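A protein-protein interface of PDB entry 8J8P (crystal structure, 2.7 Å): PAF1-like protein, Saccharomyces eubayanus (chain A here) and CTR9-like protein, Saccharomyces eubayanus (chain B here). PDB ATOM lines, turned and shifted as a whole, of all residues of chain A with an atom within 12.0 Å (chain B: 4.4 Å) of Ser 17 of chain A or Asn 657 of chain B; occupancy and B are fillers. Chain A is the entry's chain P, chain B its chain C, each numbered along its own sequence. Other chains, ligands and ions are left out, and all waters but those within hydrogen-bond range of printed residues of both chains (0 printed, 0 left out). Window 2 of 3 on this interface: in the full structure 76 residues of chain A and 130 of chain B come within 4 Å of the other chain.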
ATOM      1  N   SER A  17     -29.828  27.235  11.897  1.00  0.00           N
ATOM      2  CA  SER A  17     -31.064  27.135  11.132  1.00  0.00           C
ATOM      3  C   SER A  17     -30.892  27.670   9.714  1.00  0.00           C
ATOM      4  O   SER A  17     -29.781  27.658   9.177  1.00  0.00           O
ATOM      5  CB  SER A  17     -32.185  27.878  11.847  1.00  0.00           C
ATOM      6  OG  SER A  17     -32.308  27.390  13.168  1.00  0.00           O
ATOM      7  N   LEU A  18     -31.999  28.146   9.119  1.00  0.00           N
ATOM      8  CA  LEU A  18     -32.062  28.487   7.702  1.00  0.00           C
ATOM      9  C   LEU A  18     -33.400  29.143   7.362  1.00  0.00           C
ATOM     10  O   LEU A  18     -34.437  28.773   7.929  1.00  0.00           O
ATOM     11  CB  LEU A  18     -31.862  27.226   6.857  1.00  0.00           C
ATOM     12  CG  LEU A  18     -31.372  27.283   5.409  1.00  0.00           C
ATOM     13  CD1 LEU A  18     -30.127  28.139   5.278  1.00  0.00           C
ATOM     14  CD2 LEU A  18     -31.106  25.869   4.906  1.00  0.00           C
ATOM     15  N   PRO A  19     -33.425  30.124   6.440  1.00  0.00           N
ATOM     16  CA  PRO A  19     -34.706  30.700   6.026  1.00  0.00           C
ATOM     17  C   PRO A  19     -35.241  30.035   4.771  1.00  0.00           C
ATOM     18  O   PRO A  19     -34.585  29.166   4.180  1.00  0.00           O
ATOM     19  CB  PRO A  19     -34.350  32.167   5.768  1.00  0.00           C
ATOM     20  CG  PRO A  19     -32.968  32.074   5.184  1.00  0.00           C
ATOM     21  CD  PRO A  19     -32.306  30.828   5.787  1.00  0.00           C
ATOM     22  N   VAL A  20     -36.430  30.454   4.358  1.00  0.00           N
ATOM     23  CA  VAL A  20     -37.056  29.949   3.138  1.00  0.00           C
ATOM     24  C   VAL A  20     -36.421  30.640   1.935  1.00  0.00           C
ATOM     25  O   VAL A  20     -36.108  31.837   2.025  1.00  0.00           O
ATOM     26  CB  VAL A  20     -38.580  30.157   3.192  1.00  0.00           C
ATOM     27  CG1 VAL A  20     -38.930  31.595   3.612  1.00  0.00           C
ATOM     28  CG2 VAL A  20     -39.237  29.753   1.873  1.00  0.00           C
ATOM     29  N   PRO A  21     -36.160  29.941   0.799  1.00  0.00           N
ATOM     30  CA  PRO A  21     -35.603  30.644  -0.373  1.00  0.00           C
ATOM     31  C   PRO A  21     -36.478  31.799  -0.856  1.00  0.00           C
ATOM     32  O   PRO A  21     -37.615  31.625  -1.304  1.00  0.00           O
ATOM     33  CB  PRO A  21     -35.450  29.535  -1.425  1.00  0.00           C
ATOM     34  CG  PRO A  21     -36.236  28.372  -0.924  1.00  0.00           C
ATOM     35  CD  PRO A  21     -36.225  28.482   0.589  1.00  0.00           C
ATOM     36  N   GLN A  22     -35.924  32.998  -0.730  1.00  0.00           N
ATOM     37  CA  GLN A  22     -36.606  34.261  -0.969  1.00  0.00           C
ATOM     38  C   GLN A  22     -36.463  34.660  -2.432  1.00  0.00           C
ATOM     39  O   GLN A  22     -35.356  34.669  -2.979  1.00  0.00           O
ATOM     40  CB  GLN A  22     -36.035  35.354  -0.057  1.00  0.00           C
ATOM     41  CG  GLN A  22     -34.548  35.726  -0.284  1.00  0.00           C
ATOM     42  CD  GLN A  22     -33.535  34.572  -0.103  1.00  0.00           C
ATOM     43  OE1 GLN A  22     -33.883  33.391  -0.132  1.00  0.00           O
ATOM     44  NE2 GLN A  22     -32.268  34.932   0.067  1.00  0.00           N
ATOM     45  N   ILE B 653     -23.577  26.391   3.391  1.00  0.00           N
ATOM     46  CA  ILE B 653     -23.816  26.469   4.829  1.00  0.00           C
ATOM     47  C   ILE B 653     -24.884  25.477   5.275  1.00  0.00           C
ATOM     48  O   ILE B 653     -24.903  25.080   6.447  1.00  0.00           O
ATOM     49  CB  ILE B 653     -24.177  27.904   5.267  1.00  0.00           C
ATOM     50  CG1 ILE B 653     -25.562  28.311   4.759  1.00  0.00           C
ATOM     51  CG2 ILE B 653     -23.105  28.893   4.814  1.00  0.00           C
ATOM     52  CD1 ILE B 653     -26.632  28.318   5.827  1.00  0.00           C
ATOM     53  N   SER B 654     -25.769  25.041   4.374  1.00  0.00           N
ATOM     54  CA  SER B 654     -26.671  23.939   4.721  1.00  0.00           C
ATOM     55  C   SER B 654     -25.883  22.654   4.994  1.00  0.00           C
ATOM     56  O   SER B 654     -26.110  21.962   6.004  1.00  0.00           O
ATOM     57  CB  SER B 654     -27.698  23.727   3.607  1.00  0.00           C
ATOM     58  OG  SER B 654     -28.419  24.918   3.329  1.00  0.00           O
ATOM     59  N   LEU B 655     -24.953  22.319   4.090  1.00  0.00           N
ATOM     60  CA  LEU B 655     -24.033  21.206   4.322  1.00  0.00           C
ATOM     61  C   LEU B 655     -23.253  21.393   5.616  1.00  0.00           C
ATOM     62  O   LEU B 655     -23.022  20.429   6.357  1.00  0.00           O
ATOM     63  CB  LEU B 655     -23.057  21.072   3.155  1.00  0.00           C
ATOM     64  CG  LEU B 655     -23.446  20.367   1.860  1.00  0.00           C
ATOM     65  CD1 LEU B 655     -22.264  20.433   0.906  1.00  0.00           C
ATOM     66  CD2 LEU B 655     -23.858  18.927   2.118  1.00  0.00           C
ATOM     67  N   ALA B 656     -22.795  22.621   5.872  1.00  0.00           N
ATOM     68  CA  ALA B 656     -22.141  22.939   7.137  1.00  0.00           C
ATOM     69  C   ALA B 656     -22.996  22.526   8.321  1.00  0.00           C
ATOM     70  O   ALA B 656     -22.530  21.828   9.227  1.00  0.00           O
ATOM     71  CB  ALA B 656     -21.864  24.433   7.224  1.00  0.00           C
ATOM     72  N   ASN B 657     -24.244  22.995   8.344  1.00  0.00           N
ATOM     73  CA  ASN B 657     -25.122  22.722   9.474  1.00  0.00           C
ATOM     74  C   ASN B 657     -25.310  21.221   9.676  1.00  0.00           C
ATOM     75  O   ASN B 657     -25.262  20.733  10.812  1.00  0.00           O
ATOM     76  CB  ASN B 657     -26.465  23.423   9.273  1.00  0.00           C
ATOM     77  CG  ASN B 657     -27.296  23.462  10.541  1.00  0.00           C
ATOM     78  OD1 ASN B 657     -27.947  22.480  10.900  1.00  0.00           O
ATOM     79  ND2 ASN B 657     -27.281  24.601  11.227  1.00  0.00           N
ATOM     80  N   LEU B 658     -25.489  20.465   8.586  1.00  0.00           N
ATOM     81  CA  LEU B 658     -25.637  19.015   8.746  1.00  0.00           C
ATOM     82  C   LEU B 658     -24.358  18.379   9.292  1.00  0.00           C
ATOM     83  O   LEU B 658     -24.407  17.562  10.227  1.00  0.00           O
ATOM     84  CB  LEU B 658     -26.048  18.364   7.419  1.00  0.00           C
ATOM     85  CG  LEU B 658     -26.335  16.850   7.334  1.00  0.00           C
ATOM     86  CD1 LEU B 658     -25.091  15.972   7.211  1.00  0.00           C
ATOM     87  CD2 LEU B 658     -27.167  16.409   8.533  1.00  0.00           C
ATOM     88  N   TYR B 659     -23.203  18.728   8.715  1.00  0.00           N
ATOM     89  CA  TYR B 659     -21.957  18.094   9.126  1.00  0.00           C
ATOM     90  C   TYR B 659     -21.527  18.510  10.527  1.00  0.00           C
ATOM     91  O   TYR B 659     -20.713  17.813  11.139  1.00  0.00           O
ATOM     92  CB  TYR B 659     -20.851  18.391   8.108  1.00  0.00           C
ATOM     93  CG  TYR B 659     -20.671  17.286   7.081  1.00  0.00           C
ATOM     94  CD1 TYR B 659     -20.403  17.579   5.750  1.00  0.00           C
ATOM     95  CD2 TYR B 659     -20.781  15.949   7.446  1.00  0.00           C
ATOM     96  CE1 TYR B 659     -20.242  16.567   4.811  1.00  0.00           C
ATOM     97  CE2 TYR B 659     -20.624  14.932   6.516  1.00  0.00           C
ATOM     98  CZ  TYR B 659     -20.354  15.247   5.202  1.00  0.00           C
ATOM     99  OH  TYR B 659     -20.196  14.238   4.277  1.00  0.00           O
ATOM    100  N   VAL B 660     -22.054  19.617  11.054  1.00  0.00           N
ATOM    101  CA  VAL B 660     -21.819  19.905  12.467  1.00  0.00           C
ATOM    102  C   VAL B 660     -22.849  19.196  13.343  1.00  0.00           C
ATOM    103  O   VAL B 660     -22.546  18.836  14.486  1.00  0.00           O
ATOM    104  CB  VAL B 660     -21.794  21.420  12.751  1.00  0.00           C
ATOM    105  CG1 VAL B 660     -20.952  22.134  11.733  1.00  0.00           C
ATOM    106  CG2 VAL B 660     -23.199  22.006  12.799  1.00  0.00           C
ATOM    107  N   THR B 661     -24.068  18.973  12.835  1.00  0.00           N
ATOM    108  CA  THR B 661     -25.044  18.205  13.604  1.00  0.00           C
ATOM    109  C   THR B 661     -24.578  16.770  13.806  1.00  0.00           C
ATOM    110  O   THR B 661     -24.941  16.133  14.803  1.00  0.00           O
ATOM    111  CB  THR B 661     -26.406  18.223  12.908  1.00  0.00           C
ATOM    112  OG1 THR B 661     -26.634  19.510  12.321  1.00  0.00           O
ATOM    113  CG2 THR B 661     -27.517  17.925  13.906  1.00  0.00           C
ATOM    114  N   TYR B 689     -16.982  27.229   7.041  1.00  0.00           N
ATOM    115  CA  TYR B 689     -17.531  28.505   7.490  1.00  0.00           C
ATOM    116  C   TYR B 689     -16.534  29.631   7.269  1.00  0.00           C
ATOM    117  O   TYR B 689     -16.920  30.775   7.002  1.00  0.00           O
ATOM    118  CB  TYR B 689     -17.906  28.437   8.971  1.00  0.00           C
ATOM    119  CG  TYR B 689     -19.214  27.750   9.296  1.00  0.00           C
ATOM    120  CD1 TYR B 689     -20.426  28.409   9.144  1.00  0.00           C
ATOM    121  CD2 TYR B 689     -19.232  26.455   9.795  1.00  0.00           C
ATOM    122  CE1 TYR B 689     -21.622  27.788   9.459  1.00  0.00           C
ATOM    123  CE2 TYR B 689     -20.420  25.825  10.114  1.00  0.00           C
ATOM    124  CZ  TYR B 689     -21.613  26.494   9.945  1.00  0.00           C
ATOM    125  OH  TYR B 689     -22.800  25.871  10.258  1.00  0.00           O
ATOM    126  N   PHE B 701     -25.774  34.171   8.872  1.00  0.00           N
ATOM    127  CA  PHE B 701     -25.986  32.819   9.371  1.00  0.00           C
ATOM    128  C   PHE B 701     -24.677  32.071   9.611  1.00  0.00           C
ATOM    129  O   PHE B 701     -24.604  31.242  10.525  1.00  0.00           O
ATOM    130  CB  PHE B 701     -26.900  32.050   8.415  1.00  0.00           C
ATOM    131  CG  PHE B 701     -28.335  32.533   8.424  1.00  0.00           C
ATOM    132  CD1 PHE B 701     -29.395  31.643   8.362  1.00  0.00           C
ATOM    133  CD2 PHE B 701     -28.617  33.885   8.498  1.00  0.00           C
ATOM    134  CE1 PHE B 701     -30.703  32.105   8.386  1.00  0.00           C
ATOM    135  CE2 PHE B 701     -29.913  34.350   8.515  1.00  0.00           C
ATOM    136  CZ  PHE B 701     -30.962  33.460   8.455  1.00  0.00           C
ATOM    137  N   GLN B 704     -24.128  32.756  13.018  1.00  0.00           N
ATOM    138  CA  GLN B 704     -24.750  31.855  13.979  1.00  0.00           C
ATOM    139  C   GLN B 704     -24.124  30.468  13.935  1.00  0.00           C
ATOM    140  O   GLN B 704     -24.190  29.748  14.937  1.00  0.00           O
ATOM    141  CB  GLN B 704     -26.271  31.772  13.790  1.00  0.00           C
ATOM    142  CG  GLN B 704     -26.738  31.240  12.466  1.00  0.00           C
ATOM    143  CD  GLN B 704     -27.930  30.321  12.570  1.00  0.00           C
ATOM    144  OE1 GLN B 704     -28.923  30.638  13.228  1.00  0.00           O
ATOM    145  NE2 GLN B 704     -27.841  29.171  11.908  1.00  0.00           N
ATOM    146  N   ASP B 734     -35.187  31.650  15.577  1.00  0.00           N
ATOM    147  CA  ASP B 734     -34.136  30.691  15.884  1.00  0.00           C
ATOM    148  C   ASP B 734     -32.948  31.378  16.544  1.00  0.00           C
ATOM    149  O   ASP B 734     -32.516  30.964  17.618  1.00  0.00           O
ATOM    150  CB  ASP B 734     -33.711  29.928  14.631  1.00  0.00           C
ATOM    151  CG  ASP B 734     -34.467  28.620  14.467  1.00  0.00           C
ATOM    152  OD1 ASP B 734     -35.234  28.524  13.489  1.00  0.00           O
ATOM    153  OD2 ASP B 734     -34.286  27.693  15.288  1.00  0.00           O
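The side-chain amide nitrogen (NE2) of Gln 704 of chain B lies close to the backbone NH (N) of Ser 17 of chain A, 2.8 Å away. OD2 of Asp 734 of chain B lies close to OG of Ser 17 of chain A (2.9 Å).
Among the printed residues, pairs that only touch across the chains: Ser 17 of chain A with Asn 657 of chain B (3.7 Å), Leu 18 of chain A with Ile 653 of chain B (3.5 Å), Leu 18 of chain A with Ser 654 of chain B (3.3 Å), Leu 18 of chain A with Phe 701 of chain B (3.9 Å) and Pro 19 of chain A with Phe 701 of chain B (3.3 Å).
Asn 657 of chain B touches one residue of chain A. Ile 653 of chain B touches one residue of chain A. No residue of chain A comes within 4 Å of Ala 656 of chain B. No residue of chain A comes within 4 Å of Val 660 of chain B. No residue of chain A comes within 4 Å of Thr 661 of chain B. Asp 734 of chain B touches one residue of chain A. Printed residues of chain A within 4 Å of Gln 704 of chain B: Ser 17 (2.8 Å). Printed residues of chain B within 4 Å of Leu 18 of chain A: Ile 653, Ser 654 and Phe 701. Of the printed residues of chain B, Pro 19 of chain A touches Phe 701 (3.3 Å). Tyr 689 of chain B touches none of the printed residues of chain A. The nearest residue of chain B that does not touch Ser 17 of chain A is Phe 701 of chain B (4.1 Å).
Of the 13 printed residues of chain B, 6 touch a printed residue of chain A. Printed residues of chain B that touch a printed residue of chain A: Ile 653, Ser 654, Asn 657, Phe 701, Gln 704 and Asp 734. Among the printed residues, 7 pairs touch across the chains.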
